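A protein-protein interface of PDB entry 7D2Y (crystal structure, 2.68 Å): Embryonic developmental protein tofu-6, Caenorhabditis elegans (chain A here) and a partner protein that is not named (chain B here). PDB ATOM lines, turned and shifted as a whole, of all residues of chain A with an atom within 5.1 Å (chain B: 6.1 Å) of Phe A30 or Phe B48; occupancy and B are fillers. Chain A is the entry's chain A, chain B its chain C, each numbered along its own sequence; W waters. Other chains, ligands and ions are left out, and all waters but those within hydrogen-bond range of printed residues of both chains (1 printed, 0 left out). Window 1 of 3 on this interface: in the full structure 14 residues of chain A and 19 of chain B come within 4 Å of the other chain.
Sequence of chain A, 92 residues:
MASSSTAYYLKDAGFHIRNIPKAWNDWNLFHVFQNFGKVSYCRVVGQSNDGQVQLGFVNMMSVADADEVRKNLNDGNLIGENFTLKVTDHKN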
ATOM      1  N   ASP A  26      27.097 -27.543  11.013  1.00  0.00           N
ATOM      2  CA  ASP A  26      26.369 -26.363  10.582  1.00  0.00           C
ATOM      3  C   ASP A  26      26.380 -26.208   9.066  1.00  0.00           C
ATOM      4  O   ASP A  26      25.468 -25.594   8.503  1.00  0.00           O
ATOM      5  CB  ASP A  26      26.946 -25.130  11.265  1.00  0.00           C
ATOM      6  CG  ASP A  26      28.447 -25.028  11.108  1.00  0.00           C
ATOM      7  OD1 ASP A  26      29.034 -25.946  10.483  1.00  0.00           O
ATOM      8  OD2 ASP A  26      29.034 -24.030  11.608  1.00  0.00           O
ATOM      9  N   TRP A  27      27.383 -26.745   8.376  1.00  0.00           N
ATOM     10  CA  TRP A  27      27.366 -26.609   6.925  1.00  0.00           C
ATOM     11  C   TRP A  27      26.220 -27.395   6.321  1.00  0.00           C
ATOM     12  O   TRP A  27      25.520 -26.887   5.437  1.00  0.00           O
ATOM     13  CB  TRP A  27      28.696 -27.041   6.319  1.00  0.00           C
ATOM     14  CG  TRP A  27      29.698 -25.939   6.345  1.00  0.00           C
ATOM     15  CD1 TRP A  27      30.751 -25.816   7.195  1.00  0.00           C
ATOM     16  CD2 TRP A  27      29.724 -24.775   5.500  1.00  0.00           C
ATOM     17  NE1 TRP A  27      31.440 -24.658   6.928  1.00  0.00           N
ATOM     18  CE2 TRP A  27      30.827 -24.001   5.892  1.00  0.00           C
ATOM     19  CE3 TRP A  27      28.913 -24.314   4.453  1.00  0.00           C
ATOM     20  CZ2 TRP A  27      31.150 -22.788   5.270  1.00  0.00           C
ATOM     21  CZ3 TRP A  27      29.230 -23.118   3.840  1.00  0.00           C
ATOM     22  CH2 TRP A  27      30.338 -22.369   4.243  1.00  0.00           C
ATOM     23  N   ASN A  28      26.015 -28.634   6.789  1.00  0.00           N
ATOM     24  CA  ASN A  28      24.875 -29.431   6.359  1.00  0.00           C
ATOM     25  C   ASN A  28      23.582 -28.657   6.545  1.00  0.00           C
ATOM     26  O   ASN A  28      22.822 -28.452   5.594  1.00  0.00           O
ATOM     27  CB  ASN A  28      24.810 -30.738   7.154  1.00  0.00           C
ATOM     28  CG  ASN A  28      25.754 -31.786   6.635  1.00  0.00           C
ATOM     29  OD1 ASN A  28      26.664 -32.230   7.344  1.00  0.00           O
ATOM     30  ND2 ASN A  28      25.548 -32.192   5.386  1.00  0.00           N
ATOM     31  N   LEU A  29      23.322 -28.227   7.782  1.00  0.00           N
ATOM     32  CA  LEU A  29      22.110 -27.477   8.076  1.00  0.00           C
ATOM     33  C   LEU A  29      21.965 -26.292   7.135  1.00  0.00           C
ATOM     34  O   LEU A  29      20.892 -26.060   6.565  1.00  0.00           O
ATOM     35  CB  LEU A  29      22.130 -27.016   9.531  1.00  0.00           C
ATOM     36  CG  LEU A  29      20.861 -26.320  10.020  1.00  0.00           C
ATOM     37  CD1 LEU A  29      19.593 -27.136   9.690  1.00  0.00           C
ATOM     38  CD2 LEU A  29      20.977 -26.045  11.501  1.00  0.00           C
ATOM     39  N   PHE A  30      23.057 -25.551   6.942  1.00  0.00           N
ATOM     40  CA  PHE A  30      23.031 -24.386   6.068  1.00  0.00           C
ATOM     41  C   PHE A  30      22.603 -24.766   4.655  1.00  0.00           C
ATOM     42  O   PHE A  30      21.675 -24.169   4.089  1.00  0.00           O
ATOM     43  CB  PHE A  30      24.403 -23.719   6.065  1.00  0.00           C
ATOM     44  CG  PHE A  30      24.604 -22.763   4.935  1.00  0.00           C
ATOM     45  CD1 PHE A  30      24.087 -21.483   4.995  1.00  0.00           C
ATOM     46  CD2 PHE A  30      25.306 -23.144   3.806  1.00  0.00           C
ATOM     47  CE1 PHE A  30      24.255 -20.612   3.954  1.00  0.00           C
ATOM     48  CE2 PHE A  30      25.474 -22.273   2.755  1.00  0.00           C
ATOM     49  CZ  PHE A  30      24.951 -21.005   2.829  1.00  0.00           C
ATOM     50  N   HIS A  31      23.259 -25.770   4.068  1.00  0.00           N
ATOM     51  CA  HIS A  31      22.982 -26.103   2.676  1.00  0.00           C
ATOM     52  C   HIS A  31      21.539 -26.515   2.474  1.00  0.00           C
ATOM     53  O   HIS A  31      20.983 -26.319   1.385  1.00  0.00           O
ATOM     54  CB  HIS A  31      23.923 -27.196   2.195  1.00  0.00           C
ATOM     55  CG  HIS A  31      25.233 -26.666   1.719  1.00  0.00           C
ATOM     56  ND1 HIS A  31      25.326 -25.713   0.726  1.00  0.00           N
ATOM     57  CD2 HIS A  31      26.500 -26.925   2.116  1.00  0.00           C
ATOM     58  CE1 HIS A  31      26.595 -25.423   0.519  1.00  0.00           C
ATOM     59  NE2 HIS A  31      27.330 -26.145   1.348  1.00  0.00           N
ATOM     60  N   VAL A  32      20.911 -27.074   3.505  1.00  0.00           N
ATOM     61  CA  VAL A  32      19.497 -27.384   3.404  1.00  0.00           C
ATOM     62  C   VAL A  32      18.704 -26.107   3.198  1.00  0.00           C
ATOM     63  O   VAL A  32      17.891 -26.004   2.272  1.00  0.00           O
ATOM     64  CB  VAL A  32      19.025 -28.153   4.646  1.00  0.00           C
ATOM     65  CG1 VAL A  32      17.504 -28.292   4.647  1.00  0.00           C
ATOM     66  CG2 VAL A  32      19.724 -29.501   4.710  1.00  0.00           C
ATOM     67  N   PHE A  33      18.945 -25.098   4.033  1.00  0.00           N
ATOM     68  CA  PHE A  33      18.122 -23.907   3.913  1.00  0.00           C
ATOM     69  C   PHE A  33      18.565 -22.993   2.781  1.00  0.00           C
ATOM     70  O   PHE A  33      17.773 -22.151   2.344  1.00  0.00           O
ATOM     71  CB  PHE A  33      18.069 -23.171   5.245  1.00  0.00           C
ATOM     72  CG  PHE A  33      17.126 -23.806   6.214  1.00  0.00           C
ATOM     73  CD1 PHE A  33      17.463 -24.990   6.848  1.00  0.00           C
ATOM     74  CD2 PHE A  33      15.881 -23.263   6.452  1.00  0.00           C
ATOM     75  CE1 PHE A  33      16.586 -25.605   7.709  1.00  0.00           C
ATOM     76  CE2 PHE A  33      15.007 -23.872   7.321  1.00  0.00           C
ATOM     77  CZ  PHE A  33      15.358 -25.041   7.944  1.00  0.00           C
ATOM     78  N   GLN A  34      19.776 -23.173   2.251  1.00  0.00           N
ATOM     79  CA  GLN A  34      20.200 -22.317   1.150  1.00  0.00           C
ATOM     80  C   GLN A  34      19.426 -22.616  -0.126  1.00  0.00           C
ATOM     81  O   GLN A  34      19.270 -21.730  -0.973  1.00  0.00           O
ATOM     82  CB  GLN A  34      21.695 -22.466   0.901  1.00  0.00           C
ATOM     83  CG  GLN A  34      22.211 -21.422  -0.047  1.00  0.00           C
ATOM     84  CD  GLN A  34      23.626 -21.683  -0.506  1.00  0.00           C
ATOM     85  OE1 GLN A  34      24.186 -22.763  -0.286  1.00  0.00           O
ATOM     86  NE2 GLN A  34      24.222 -20.686  -1.151  1.00  0.00           N
ATOM     87  N   VAL A  39      20.810 -17.070   3.492  1.00  0.00           N
ATOM     88  CA  VAL A  39      20.803 -17.406   4.911  1.00  0.00           C
ATOM     89  C   VAL A  39      21.643 -16.386   5.669  1.00  0.00           C
ATOM     90  O   VAL A  39      22.736 -16.030   5.226  1.00  0.00           O
ATOM     91  CB  VAL A  39      21.314 -18.845   5.158  1.00  0.00           C
ATOM     92  CG1 VAL A  39      21.286 -19.176   6.626  1.00  0.00           C
ATOM     93  CG2 VAL A  39      20.480 -19.848   4.385  1.00  0.00           C
ATOM     94  N   CYS A  42      23.122 -19.503  10.938  1.00  0.00           N
ATOM     95  CA  CYS A  42      22.884 -20.934  10.881  1.00  0.00           C
ATOM     96  C   CYS A  42      23.764 -21.593  11.925  1.00  0.00           C
ATOM     97  O   CYS A  42      24.988 -21.427  11.918  1.00  0.00           O
ATOM     98  CB  CYS A  42      23.180 -21.491   9.502  1.00  0.00           C
ATOM     99  SG  CYS A  42      22.962 -23.269   9.458  1.00  0.00           S
ATOM    100  N   GLU B   3      37.297 -16.199   9.099  1.00  0.00           N
ATOM    101  CA  GLU B   3      36.264 -16.618   8.171  1.00  0.00           C
ATOM    102  C   GLU B   3      35.105 -15.633   8.061  1.00  0.00           C
ATOM    103  O   GLU B   3      34.111 -15.960   7.414  1.00  0.00           O
ATOM    104  CB  GLU B   3      35.743 -18.004   8.559  1.00  0.00           C
ATOM    105  CG  GLU B   3      36.598 -19.169   8.036  1.00  0.00           C
ATOM    106  CD  GLU B   3      36.019 -20.543   8.392  1.00  0.00           C
ATOM    107  OE1 GLU B   3      35.605 -21.307   7.473  1.00  0.00           O
ATOM    108  OE2 GLU B   3      35.975 -20.847   9.605  1.00  0.00           O
ATOM    109  N   TYR B  27      23.955  -8.653   2.405  1.00  0.00           N
ATOM    110  CA  TYR B  27      24.708  -9.236   3.515  1.00  0.00           C
ATOM    111  C   TYR B  27      25.126  -8.185   4.543  1.00  0.00           C
ATOM    112  O   TYR B  27      25.345  -7.024   4.214  1.00  0.00           O
ATOM    113  CB  TYR B  27      25.942  -9.961   2.977  1.00  0.00           C
ATOM    114  CG  TYR B  27      25.507 -11.032   2.027  1.00  0.00           C
ATOM    115  CD1 TYR B  27      24.780 -12.110   2.485  1.00  0.00           C
ATOM    116  CD2 TYR B  27      25.744 -10.922   0.666  1.00  0.00           C
ATOM    117  CE1 TYR B  27      24.336 -13.066   1.644  1.00  0.00           C
ATOM    118  CE2 TYR B  27      25.315 -11.883  -0.191  1.00  0.00           C
ATOM    119  CZ  TYR B  27      24.602 -12.961   0.312  1.00  0.00           C
ATOM    120  OH  TYR B  27      24.129 -13.940  -0.519  1.00  0.00           O
ATOM    121  N   ASN B  46      29.285 -13.478   9.256  1.00  0.00           N
ATOM    122  CA  ASN B  46      29.762 -14.821   9.578  1.00  0.00           C
ATOM    123  C   ASN B  46      30.142 -15.523   8.284  1.00  0.00           C
ATOM    124  O   ASN B  46      29.938 -14.996   7.186  1.00  0.00           O
ATOM    125  CB  ASN B  46      28.719 -15.627  10.358  1.00  0.00           C
ATOM    126  CG  ASN B  46      27.378 -15.711   9.638  1.00  0.00           C
ATOM    127  OD1 ASN B  46      27.292 -16.187   8.505  1.00  0.00           O
ATOM    128  ND2 ASN B  46      26.322 -15.258  10.304  1.00  0.00           N
ATOM    129  N   LYS B  47      30.704 -16.731   8.428  1.00  0.00           N
ATOM    130  CA  LYS B  47      31.231 -17.475   7.282  1.00  0.00           C
ATOM    131  C   LYS B  47      30.156 -17.803   6.250  1.00  0.00           C
ATOM    132  O   LYS B  47      30.460 -17.952   5.058  1.00  0.00           O
ATOM    133  CB  LYS B  47      31.870 -18.767   7.755  1.00  0.00           C
ATOM    134  CG  LYS B  47      30.885 -19.701   8.379  1.00  0.00           C
ATOM    135  CD  LYS B  47      31.593 -20.779   9.147  1.00  0.00           C
ATOM    136  CE  LYS B  47      30.629 -21.580  10.034  1.00  0.00           C
ATOM    137  NZ  LYS B  47      31.362 -22.462  10.966  1.00  0.00           N
ATOM    138  N   PHE B  48      28.902 -17.932   6.682  1.00  0.00           N
ATOM    139  CA  PHE B  48      27.857 -18.265   5.734  1.00  0.00           C
ATOM    140  C   PHE B  48      27.534 -17.069   4.853  1.00  0.00           C
ATOM    141  O   PHE B  48      27.334 -17.208   3.636  1.00  0.00           O
ATOM    142  CB  PHE B  48      26.635 -18.771   6.486  1.00  0.00           C
ATOM    143  CG  PHE B  48      26.909 -20.009   7.289  1.00  0.00           C
ATOM    144  CD1 PHE B  48      27.373 -21.166   6.665  1.00  0.00           C
ATOM    145  CD2 PHE B  48      26.723 -20.024   8.661  1.00  0.00           C
ATOM    146  CE1 PHE B  48      27.636 -22.332   7.417  1.00  0.00           C
ATOM    147  CE2 PHE B  48      26.980 -21.193   9.416  1.00  0.00           C
ATOM    148  CZ  PHE B  48      27.439 -22.340   8.791  1.00  0.00           C
ATOM    149  N   GLN B  49      27.551 -15.872   5.420  1.00  0.00           N
ATOM    150  CA  GLN B  49      27.344 -14.735   4.541  1.00  0.00           C
ATOM    151  C   GLN B  49      28.537 -14.545   3.640  1.00  0.00           C
ATOM    152  O   GLN B  49      28.370 -14.244   2.459  1.00  0.00           O
ATOM    153  CB  GLN B  49      27.007 -13.484   5.348  1.00  0.00           C
ATOM    154  CG  GLN B  49      25.681 -13.666   6.084  1.00  0.00           C
ATOM    155  CD  GLN B  49      25.138 -12.378   6.626  1.00  0.00           C
ATOM    156  OE1 GLN B  49      25.316 -11.318   6.034  1.00  0.00           O
ATOM    157  NE2 GLN B  49      24.469 -12.455   7.762  1.00  0.00           N
ATOM    158  N   VAL B  50      29.744 -14.789   4.146  1.00  0.00           N
ATOM    159  CA  VAL B  50      30.927 -14.686   3.282  1.00  0.00           C
ATOM    160  C   VAL B  50      30.830 -15.683   2.132  1.00  0.00           C
ATOM    161  O   VAL B  50      31.048 -15.346   0.961  1.00  0.00           O
ATOM    162  CB  VAL B  50      32.210 -14.918   4.086  1.00  0.00           C
ATOM    163  CG1 VAL B  50      33.370 -15.002   3.128  1.00  0.00           C
ATOM    164  CG2 VAL B  50      32.408 -13.822   5.090  1.00  0.00           C
ATOM    165  N   TYR B  51      30.492 -16.931   2.459  1.00  0.00           N
ATOM    166  CA  TYR B  51      30.363 -17.966   1.451  1.00  0.00           C
ATOM    167  C   TYR B  51      29.370 -17.562   0.365  1.00  0.00           C
ATOM    168  O   TYR B  51      29.658 -17.681  -0.834  1.00  0.00           O
ATOM    169  CB  TYR B  51      29.940 -19.264   2.132  1.00  0.00           C
ATOM    170  CG  TYR B  51      29.700 -20.402   1.181  1.00  0.00           C
ATOM    171  CD1 TYR B  51      30.760 -21.160   0.691  1.00  0.00           C
ATOM    172  CD2 TYR B  51      28.420 -20.706   0.762  1.00  0.00           C
ATOM    173  CE1 TYR B  51      30.549 -22.178  -0.186  1.00  0.00           C
ATOM    174  CE2 TYR B  51      28.201 -21.718  -0.119  1.00  0.00           C
ATOM    175  CZ  TYR B  51      29.265 -22.455  -0.586  1.00  0.00           C
ATOM    176  OH  TYR B  51      29.029 -23.484  -1.457  1.00  0.00           O
ATOM    177  N   GLN B  52      28.194 -17.076   0.770  1.00  0.00           N
ATOM    178  CA  GLN B  52      27.176 -16.656  -0.191  1.00  0.00           C
ATOM    179  C   GLN B  52      27.603 -15.420  -0.988  1.00  0.00           C
ATOM    180  O   GLN B  52      27.314 -15.318  -2.186  1.00  0.00           O
ATOM    181  CB  GLN B  52      25.871 -16.385   0.551  1.00  0.00           C
ATOM    182  CG  GLN B  52      25.355 -17.601   1.277  1.00  0.00           C
ATOM    183  CD  GLN B  52      24.198 -17.284   2.180  1.00  0.00           C
ATOM    184  OE1 GLN B  52      23.033 -17.376   1.784  1.00  0.00           O
ATOM    185  NE2 GLN B  52      24.507 -16.905   3.414  1.00  0.00           N
ATOM    186  N   ALA B  53      28.286 -14.464  -0.347  1.00  0.00           N
ATOM    187  CA  ALA B  53      28.722 -13.280  -1.085  1.00  0.00           C
ATOM    188  C   ALA B  53      29.718 -13.653  -2.182  1.00  0.00           C
ATOM    189  O   ALA B  53      29.588 -13.197  -3.326  1.00  0.00           O
ATOM    190  CB  ALA B  53      29.311 -12.232  -0.137  1.00  0.00           C
ATOM    191  N   VAL B  74      37.080 -19.248   2.937  1.00  0.00           N
ATOM    192  CA  VAL B  74      35.961 -20.022   3.461  1.00  0.00           C
ATOM    193  C   VAL B  74      35.635 -21.120   2.459  1.00  0.00           C
ATOM    194  O   VAL B  74      35.309 -20.838   1.300  1.00  0.00           O
ATOM    195  CB  VAL B  74      34.732 -19.134   3.743  1.00  0.00           C
ATOM    196  CG1 VAL B  74      33.498 -19.973   3.956  1.00  0.00           C
ATOM    197  CG2 VAL B  74      34.973 -18.296   4.968  1.00  0.00           C
ATOM    198  N   SER B  76      33.047 -24.383   1.955  1.00  0.00           N
ATOM    199  CA  SER B  76      31.914 -25.165   2.435  1.00  0.00           C
ATOM    200  C   SER B  76      32.388 -26.545   2.883  1.00  0.00           C
ATOM    201  O   SER B  76      33.032 -27.266   2.117  1.00  0.00           O
ATOM    202  CB  SER B  76      30.878 -25.279   1.325  1.00  0.00           C
ATOM    203  OG  SER B  76      29.922 -26.289   1.607  1.00  0.00           O
HETATM  204  O   HOH W   1      31.630 -25.887  11.125  1.00  0.00           O
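The side-chain carboxylate of Asp A26 is in salt-bridge range of the side-chain amino group of Lys B47, at 2.9 Å. A ring nitrogen (NE2) of His A31 lies within hydrogen-bond range of the side-chain hydroxyl (OG) of Ser B76, 2.6 Å away. The side-chain amide nitrogen of Gln B52 sits at hydrogen-bond distance from the backbone carbonyl oxygen of Val A39.
O of Asp A26 sits at hydrogen-bond distance from SG of Cys A42, 3.5 Å away. The backbone NH (N) of Phe A30 is in hydrogen-bond range of the side-chain sulfur (SG) of Cys A42 (3.4 Å). OE1 of Gln A34 is in hydrogen-bond range of ND1 of His A31 (3.3 Å). The backbone NH (N) of Phe B48 is in hydrogen-bond range of the side-chain amide oxygen (OD1) of Asn B46. OD1 of Asn B46 lies within hydrogen-bond range of N of Gln B49. The side-chain amide nitrogen (NE2) of Gln B52 is in hydrogen-bond range of the backbone carbonyl oxygen (O) of Phe B48, at 2.9 Å.
Asp A26 touches Phe B48. Trp A27 touches Phe B48. CH2 of Trp A27 touches CG of Tyr B51, 3.7 Å away. CZ2 of Trp A27 touches CG1 of Val B74, 3.9 Å away. Trp A27 touches Ser B76 (CE3 to OG, 3.6 Å). CD1 of Phe B48 touches CG of Phe A30, at 3.6 Å. Phe A30 touches Tyr B51. NE2 of Gln B52 touches CE1 of Phe A30, at 3.8 Å. OH of Tyr B51 touches CE1 of His A31, 3.7 Å away. Gln B49 touches Val A39 (CG to O, 3.9 Å).
Of the printed residues of chain B, Asp A26 touches Lys B47 and Phe B48. Printed residues of chain B within 4 Å of Trp A27: Phe B48 (3.7 Å), Tyr B51 (3.7 Å), Val B74 (3.9 Å) and Ser B76 (3.6 Å). Phe A30 touches just these residues of chain B: Phe B48 (3.6 Å), Tyr B51 (3.9 Å) and Gln B52 (3.8 Å). Phe B48 touches just these residues of chain A: Asp A26 (3.7 Å), Trp A27 (3.7 Å), Phe A30 (3.6 Å) and Cys A42 (3.2 Å). The nearest residue of chain A that does not touch Phe B48 is Val A39 (4.9 Å).
Of the 11 printed residues of chain A, 6 touch a printed residue of chain B. Printed residues of chain A that touch a printed residue of chain B: Asp A26, Trp A27, Phe A30, His A31, Val A39 and Cys A42. Hydrophobic or aromatic side chains of chain A within 4 Å of the printed part of chain B: Trp A27, Phe A30 and His A31. Of the 12 printed residues of chain B, 7 touch a printed residue of chain A. Printed residues of chain B that touch a printed residue of chain A: Lys B47, Phe B48, Gln B49, Tyr B51, Gln B52, Val B74 and Ser B76. Hydrophobic or aromatic side chains of chain B that line the printed part of chain A: Phe B48, Tyr B51 and Val B74.
Water W1 bridges OD1 of Asp A26 (2.7 Å) and NZ of Lys B47 (3.4 Å).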
